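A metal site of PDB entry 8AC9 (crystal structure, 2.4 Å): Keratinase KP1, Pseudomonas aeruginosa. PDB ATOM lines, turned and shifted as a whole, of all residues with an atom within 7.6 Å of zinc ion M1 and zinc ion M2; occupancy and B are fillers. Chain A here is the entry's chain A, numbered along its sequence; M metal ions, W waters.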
ATOM      1  N   HIS A 270       8.207 -23.029  20.029  1.00  0.00           N
ATOM      2  CA  HIS A 270       7.959 -22.362  18.749  1.00  0.00           C
ATOM      3  C   HIS A 270       6.955 -21.224  18.925  1.00  0.00           C
ATOM      4  O   HIS A 270       6.000 -21.309  19.709  1.00  0.00           O
ATOM      5  CB  HIS A 270       7.512 -23.361  17.663  1.00  0.00           C
ATOM      6  CG  HIS A 270       6.106 -23.866  17.776  1.00  0.00           C
ATOM      7  ND1 HIS A 270       5.028 -23.225  17.206  1.00  0.00           N
ATOM      8  CD2 HIS A 270       5.614 -25.016  18.301  1.00  0.00           C
ATOM      9  CE1 HIS A 270       3.929 -23.927  17.427  1.00  0.00           C
ATOM     10  NE2 HIS A 270       4.255 -25.020  18.082  1.00  0.00           N
ATOM     11  N   ASP A 272       5.532 -19.431  16.200  1.00  0.00           N
ATOM     12  CA  ASP A 272       4.575 -19.280  15.101  1.00  0.00           C
ATOM     13  C   ASP A 272       3.290 -20.054  15.388  1.00  0.00           C
ATOM     14  O   ASP A 272       3.282 -21.034  16.148  1.00  0.00           O
ATOM     15  CB  ASP A 272       5.151 -19.752  13.767  1.00  0.00           C
ATOM     16  CG  ASP A 272       5.524 -21.237  13.757  1.00  0.00           C
ATOM     17  OD1 ASP A 272       6.151 -21.701  14.742  1.00  0.00           O
ATOM     18  OD2 ASP A 272       5.230 -21.940  12.761  1.00  0.00           O
ATOM     19  N   SER A 273       2.218 -19.565  14.802  1.00  0.00           N
ATOM     20  CA  SER A 273       0.935 -20.234  14.769  1.00  0.00           C
ATOM     21  C   SER A 273       0.716 -20.781  13.361  1.00  0.00           C
ATOM     22  O   SER A 273       1.433 -20.419  12.438  1.00  0.00           O
ATOM     23  CB  SER A 273      -0.188 -19.257  15.119  1.00  0.00           C
ATOM     24  OG  SER A 273      -0.209 -18.243  14.121  1.00  0.00           O
ATOM     25  N   VAL A 274      -0.318 -21.610  13.195  1.00  0.00           N
ATOM     26  CA  VAL A 274      -0.792 -21.957  11.850  1.00  0.00           C
ATOM     27  C   VAL A 274      -1.434 -20.711  11.247  1.00  0.00           C
ATOM     28  O   VAL A 274      -1.665 -19.710  11.943  1.00  0.00           O
ATOM     29  CB  VAL A 274      -1.795 -23.121  11.841  1.00  0.00           C
ATOM     30  CG1 VAL A 274      -1.115 -24.450  12.201  1.00  0.00           C
ATOM     31  CG2 VAL A 274      -2.940 -22.819  12.767  1.00  0.00           C
ATOM     32  N   ASN A 281      -2.886 -21.428  22.523  1.00  0.00           N
ATOM     33  CA  ASN A 281      -2.365 -22.652  23.145  1.00  0.00           C
ATOM     34  C   ASN A 281      -1.192 -23.201  22.342  1.00  0.00           C
ATOM     35  O   ASN A 281      -0.169 -23.589  22.917  1.00  0.00           O
ATOM     36  CB  ASN A 281      -3.417 -23.763  23.319  1.00  0.00           C
ATOM     37  CG  ASN A 281      -2.863 -24.934  24.182  1.00  0.00           C
ATOM     38  OD1 ASN A 281      -2.138 -24.690  25.154  1.00  0.00           O
ATOM     39  ND2 ASN A 281      -3.150 -26.193  23.784  1.00  0.00           N
ATOM     40  N   ASP A 282      -1.353 -23.254  21.022  1.00  0.00           N
ATOM     41  CA  ASP A 282      -0.333 -23.786  20.115  1.00  0.00           C
ATOM     42  C   ASP A 282       0.245 -22.665  19.237  1.00  0.00           C
ATOM     43  O   ASP A 282      -0.286 -22.383  18.165  1.00  0.00           O
ATOM     44  CB  ASP A 282      -0.940 -24.905  19.271  1.00  0.00           C
ATOM     45  CG  ASP A 282       0.073 -25.562  18.396  1.00  0.00           C
ATOM     46  OD1 ASP A 282       1.268 -25.454  18.697  1.00  0.00           O
ATOM     47  OD2 ASP A 282      -0.321 -26.169  17.384  1.00  0.00           O
ATOM     48  N   ASN A 283       1.364 -22.069  19.666  1.00  0.00           N
ATOM     49  CA  ASN A 283       2.054 -22.417  20.906  1.00  0.00           C
ATOM     50  C   ASN A 283       2.413 -21.157  21.675  1.00  0.00           C
ATOM     51  O   ASN A 283       3.549 -21.010  22.162  1.00  0.00           O
ATOM     52  CB  ASN A 283       3.319 -23.258  20.641  1.00  0.00           C
ATOM     53  CG  ASN A 283       4.045 -23.668  21.942  1.00  0.00           C
ATOM     54  OD1 ASN A 283       3.402 -24.008  22.942  1.00  0.00           O
ATOM     55  ND2 ASN A 283       5.375 -23.608  21.926  1.00  0.00           N
ATOM     56  N   GLY A 284       1.471 -20.251  21.784  1.00  0.00           N
ATOM     57  CA  GLY A 284       1.655 -19.144  22.708  1.00  0.00           C
ATOM     58  C   GLY A 284       1.966 -19.619  24.109  1.00  0.00           C
ATOM     59  O   GLY A 284       2.752 -19.001  24.829  1.00  0.00           O
ATOM     60  N   GLU A 314       7.617 -23.568  12.773  1.00  0.00           N
ATOM     61  CA  GLU A 314       7.458 -24.944  13.209  1.00  0.00           C
ATOM     62  C   GLU A 314       6.272 -25.599  12.518  1.00  0.00           C
ATOM     63  O   GLU A 314       6.299 -26.797  12.235  1.00  0.00           O
ATOM     64  CB  GLU A 314       7.265 -25.005  14.720  1.00  0.00           C
ATOM     65  CG  GLU A 314       7.139 -26.423  15.257  1.00  0.00           C
ATOM     66  CD  GLU A 314       5.721 -26.884  15.380  1.00  0.00           C
ATOM     67  OE1 GLU A 314       4.805 -26.056  15.125  1.00  0.00           O
ATOM     68  OE2 GLU A 314       5.523 -28.074  15.726  1.00  0.00           O
ATOM     69  N   GLU A 315       5.215 -24.842  12.306  1.00  0.00           N
ATOM     70  CA  GLU A 315       4.006 -25.368  11.695  1.00  0.00           C
ATOM     71  C   GLU A 315       4.205 -25.675  10.206  1.00  0.00           C
ATOM     72  O   GLU A 315       3.369 -26.359   9.628  1.00  0.00           O
ATOM     73  CB  GLU A 315       2.860 -24.376  11.881  1.00  0.00           C
ATOM     74  CG  GLU A 315       2.598 -23.986  13.335  1.00  0.00           C
ATOM     75  CD  GLU A 315       1.911 -25.098  14.130  1.00  0.00           C
ATOM     76  OE1 GLU A 315       1.957 -26.255  13.693  1.00  0.00           O
ATOM     77  OE2 GLU A 315       1.322 -24.812  15.180  1.00  0.00           O
ATOM     78  N   ASN A 341      11.774 -28.937  25.532  1.00  0.00           N
ATOM     79  CA  ASN A 341      10.810 -28.428  24.560  1.00  0.00           C
ATOM     80  C   ASN A 341       9.465 -28.196  25.221  1.00  0.00           C
ATOM     81  O   ASN A 341       8.978 -29.061  25.967  1.00  0.00           O
ATOM     82  CB  ASN A 341      10.671 -29.398  23.384  1.00  0.00           C
ATOM     83  CG  ASN A 341       9.943 -28.783  22.245  1.00  0.00           C
ATOM     84  OD1 ASN A 341      10.384 -27.793  21.671  1.00  0.00           O
ATOM     85  ND2 ASN A 341       8.799 -29.356  21.904  1.00  0.00           N
ATOM     86  N   PHE A 342       8.855 -27.050  24.959  1.00  0.00           N
ATOM     87  CA  PHE A 342       7.550 -26.732  25.536  1.00  0.00           C
ATOM     88  C   PHE A 342       6.604 -26.296  24.425  1.00  0.00           C
ATOM     89  O   PHE A 342       6.631 -25.140  23.978  1.00  0.00           O
ATOM     90  CB  PHE A 342       7.698 -25.686  26.627  1.00  0.00           C
ATOM     91  CG  PHE A 342       8.654 -26.099  27.689  1.00  0.00           C
ATOM     92  CD1 PHE A 342       8.271 -27.046  28.631  1.00  0.00           C
ATOM     93  CD2 PHE A 342       9.961 -25.648  27.675  1.00  0.00           C
ATOM     94  CE1 PHE A 342       9.166 -27.491  29.578  1.00  0.00           C
ATOM     95  CE2 PHE A 342      10.851 -26.081  28.607  1.00  0.00           C
ATOM     96  CZ  PHE A 342      10.461 -27.005  29.568  1.00  0.00           C
ATOM     97  N   ASP A 343       5.750 -27.220  23.999  1.00  0.00           N
ATOM     98  CA  ASP A 343       4.854 -27.019  22.861  1.00  0.00           C
ATOM     99  C   ASP A 343       3.458 -27.497  23.251  1.00  0.00           C
ATOM    100  O   ASP A 343       3.202 -28.700  23.289  1.00  0.00           O
ATOM    101  CB  ASP A 343       5.383 -27.762  21.623  1.00  0.00           C
ATOM    102  CG  ASP A 343       4.588 -27.446  20.356  1.00  0.00           C
ATOM    103  OD1 ASP A 343       3.524 -26.781  20.448  1.00  0.00           O
ATOM    104  OD2 ASP A 343       5.042 -27.857  19.254  1.00  0.00           O
ATOM    105  N   MET A 344       2.566 -26.552  23.519  1.00  0.00           N
ATOM    106  CA  MET A 344       1.195 -26.831  23.943  1.00  0.00           C
ATOM    107  C   MET A 344       1.178 -27.321  25.385  1.00  0.00           C
ATOM    108  O   MET A 344       1.342 -28.527  25.643  1.00  0.00           O
ATOM    109  CB  MET A 344       0.500 -27.826  22.996  1.00  0.00           C
ATOM    110  CG  MET A 344       0.441 -27.405  21.506  1.00  0.00           C
ATOM    111  SD  MET A 344      -0.628 -28.496  20.497  1.00  0.00           S
ATOM    112  CE  MET A 344      -2.221 -28.253  21.304  1.00  0.00           C
ATOM    113  N   ARG A 396       6.847 -34.476  16.242  1.00  0.00           N
ATOM    114  CA  ARG A 396       5.945 -33.438  15.759  1.00  0.00           C
ATOM    115  C   ARG A 396       6.246 -32.074  16.365  1.00  0.00           C
ATOM    116  O   ARG A 396       5.394 -31.182  16.300  1.00  0.00           O
ATOM    117  CB  ARG A 396       4.476 -33.817  16.011  1.00  0.00           C
ATOM    118  CG  ARG A 396       3.826 -34.563  14.849  1.00  0.00           C
ATOM    119  CD  ARG A 396       2.530 -35.266  15.258  1.00  0.00           C
ATOM    120  NE  ARG A 396       1.419 -34.320  15.400  1.00  0.00           N
ATOM    121  CZ  ARG A 396       0.226 -34.647  15.884  1.00  0.00           C
ATOM    122  NH1 ARG A 396      -0.023 -35.894  16.262  1.00  0.00           N
ATOM    123  NH2 ARG A 396      -0.729 -33.729  15.979  1.00  0.00           N
ATOM    124  N   SER A 397       7.444 -31.892  16.916  1.00  0.00           N
ATOM    125  CA  SER A 397       7.840 -30.583  17.418  1.00  0.00           C
ATOM    126  C   SER A 397       9.352 -30.447  17.314  1.00  0.00           C
ATOM    127  O   SER A 397      10.043 -31.313  16.767  1.00  0.00           O
ATOM    128  CB  SER A 397       7.363 -30.383  18.865  1.00  0.00           C
ATOM    129  OG  SER A 397       7.248 -28.996  19.175  1.00  0.00           O
ATOM    130  N   ASP A 398       9.884 -29.378  17.918  1.00  0.00           N
ATOM    131  CA  ASP A 398      11.189 -28.849  17.603  1.00  0.00           C
ATOM    132  C   ASP A 398      12.342 -29.602  18.261  1.00  0.00           C
ATOM    133  O   ASP A 398      13.505 -29.302  17.982  1.00  0.00           O
ATOM    134  CB  ASP A 398      11.225 -27.378  17.982  1.00  0.00           C
ATOM    135  CG  ASP A 398      10.327 -26.540  17.083  1.00  0.00           C
ATOM    136  OD1 ASP A 398      10.617 -26.441  15.876  1.00  0.00           O
ATOM    137  OD2 ASP A 398       9.320 -26.014  17.582  1.00  0.00           O
ATOM    138  N   PHE A 413       3.719 -31.578  27.478  1.00  0.00           N
ATOM    139  CA  PHE A 413       2.683 -31.546  26.462  1.00  0.00           C
ATOM    140  C   PHE A 413       1.357 -31.777  27.182  1.00  0.00           C
ATOM    141  O   PHE A 413       1.295 -32.632  28.066  1.00  0.00           O
ATOM    142  CB  PHE A 413       2.972 -32.622  25.409  1.00  0.00           C
ATOM    143  CG  PHE A 413       1.956 -32.728  24.291  1.00  0.00           C
ATOM    144  CD1 PHE A 413       1.470 -31.602  23.661  1.00  0.00           C
ATOM    145  CD2 PHE A 413       1.518 -33.983  23.855  1.00  0.00           C
ATOM    146  CE1 PHE A 413       0.547 -31.715  22.607  1.00  0.00           C
ATOM    147  CE2 PHE A 413       0.609 -34.116  22.809  1.00  0.00           C
ATOM    148  CZ  PHE A 413       0.133 -32.989  22.177  1.00  0.00           C
ATOM    149  N   ALA A 416      -3.178 -32.631  22.053  1.00  0.00           N
ATOM    150  CA  ALA A 416      -3.699 -31.906  20.911  1.00  0.00           C
ATOM    151  C   ALA A 416      -5.000 -32.532  20.426  1.00  0.00           C
ATOM    152  O   ALA A 416      -6.021 -32.461  21.128  1.00  0.00           O
ATOM    153  CB  ALA A 416      -2.662 -31.847  19.803  1.00  0.00           C
ATOM    154  N   TYR A 440      -7.506 -27.180  18.379  1.00  0.00           N
ATOM    155  CA  TYR A 440      -6.228 -27.400  17.744  1.00  0.00           C
ATOM    156  C   TYR A 440      -6.192 -26.827  16.323  1.00  0.00           C
ATOM    157  O   TYR A 440      -7.020 -27.156  15.477  1.00  0.00           O
ATOM    158  CB  TYR A 440      -5.964 -28.908  17.742  1.00  0.00           C
ATOM    159  CG  TYR A 440      -4.657 -29.292  17.152  1.00  0.00           C
ATOM    160  CD1 TYR A 440      -3.458 -28.772  17.657  1.00  0.00           C
ATOM    161  CD2 TYR A 440      -4.599 -30.168  16.079  1.00  0.00           C
ATOM    162  CE1 TYR A 440      -2.227 -29.129  17.107  1.00  0.00           C
ATOM    163  CE2 TYR A 440      -3.371 -30.534  15.509  1.00  0.00           C
ATOM    164  CZ  TYR A 440      -2.198 -30.015  16.033  1.00  0.00           C
ATOM    165  OH  TYR A 440      -0.988 -30.358  15.485  1.00  0.00           O
ATOM    166  N   HIS A 441      -5.223 -25.947  16.066  1.00  0.00           N
ATOM    167  CA  HIS A 441      -4.975 -25.425  14.721  1.00  0.00           C
ATOM    168  C   HIS A 441      -6.198 -24.717  14.162  1.00  0.00           C
ATOM    169  O   HIS A 441      -6.412 -24.710  12.953  1.00  0.00           O
ATOM    170  CB  HIS A 441      -4.509 -26.537  13.779  1.00  0.00           C
ATOM    171  CG  HIS A 441      -3.065 -26.909  13.953  1.00  0.00           C
ATOM    172  ND1 HIS A 441      -2.373 -27.703  13.063  1.00  0.00           N
ATOM    173  CD2 HIS A 441      -2.172 -26.580  14.925  1.00  0.00           C
ATOM    174  CE1 HIS A 441      -1.121 -27.848  13.474  1.00  0.00           C
ATOM    175  NE2 HIS A 441      -0.974 -27.170  14.602  1.00  0.00           N
ATOM    176  N   ASP A 445      -8.423 -21.099  18.702  1.00  0.00           N
ATOM    177  CA  ASP A 445      -7.292 -21.321  19.625  1.00  0.00           C
ATOM    178  C   ASP A 445      -6.814 -19.967  20.142  1.00  0.00           C
ATOM    179  O   ASP A 445      -5.716 -19.489  19.850  1.00  0.00           O
ATOM    180  CB  ASP A 445      -6.151 -22.093  18.953  1.00  0.00           C
ATOM    181  CG  ASP A 445      -4.953 -22.335  19.896  1.00  0.00           C
ATOM    182  OD1 ASP A 445      -5.116 -22.121  21.123  1.00  0.00           O
ATOM    183  OD2 ASP A 445      -3.851 -22.716  19.410  1.00  0.00           O
HETATM  184 ZN    ZN M   1       2.978 -26.541  18.390  1.00  0.00          ZN
HETATM  185 ZN    ZN M   2       0.878 -26.894  15.766  1.00  0.00          ZN
HETATM  186  O   HOH W   1       1.361 -29.181  16.019  1.00  0.00           O
HETATM  187  O   HOH W   2       2.920 -27.244  16.240  1.00  0.00           O
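Zinc ion M2 is bound by water W2 (2.1 Å), the side-chain carboxylate (OD2) of Asp 282 (2.1 Å), a ring nitrogen (NE2) of His 441 (2.2 Å), the side-chain carboxylate (OE2) of Glu 315 (2.2 Å), water W1 (2.4 Å) and the side-chain carboxylate (OE1) of Glu 315 (2.4 Å).
OD2 of Asp 445 is in hydrogen-bond range of N of Asp 282 (3.0 Å). The side-chain amide nitrogen of Asn 283 lies within hydrogen-bond range of the backbone carbonyl oxygen of Phe 342 (2.9 Å). OE1 of Glu 314 lies close to NE2 of His 270. The backbone NH (N) of Glu 315 is in hydrogen-bond range of the side-chain carboxylate (OD2) of Asp 272. O of Asp 272 is in hydrogen-bond range of ND1 of His 270, 3.0 Å away. The backbone carbonyl oxygen of His 270 lies within hydrogen-bond range of the side-chain amide nitrogen of Asn 283, 3.3 Å away. N of Glu 314 is in hydrogen-bond range of OD2 of Asp 272, at 2.9 Å. N of Met 344 sits at hydrogen-bond distance from OD1 of Asn 283 (2.7 Å).
CB of Asn 283 touches zinc ion M1 (3.995 Å). Glu 314 touches zinc ion M1. Five residues have an atom within 4 Å of zinc ion M1: His 270, Asp 282, Asn 283, Glu 314 and Asp 343. Along chain A the residues within 4 Å of zinc ion M1 span positions 270 to 343.
Zinc ion M1 is bound by NE2 of His 270 (2.0 Å). The side-chain carboxylate (OD1) of Asp 282 binds zinc ion M1, 2.0 Å away. The side-chain carboxylate (OD1) of Asp 343 binds zinc ion M1. Zinc ion M1 is bound by water W2 (2.3 Å). Zinc ion M1 is bound by OD2 of Asp 343, at 2.6 Å. Zinc ion M1 has five donor atoms within binding distance.
Tyr 440 touches zinc ion M2.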
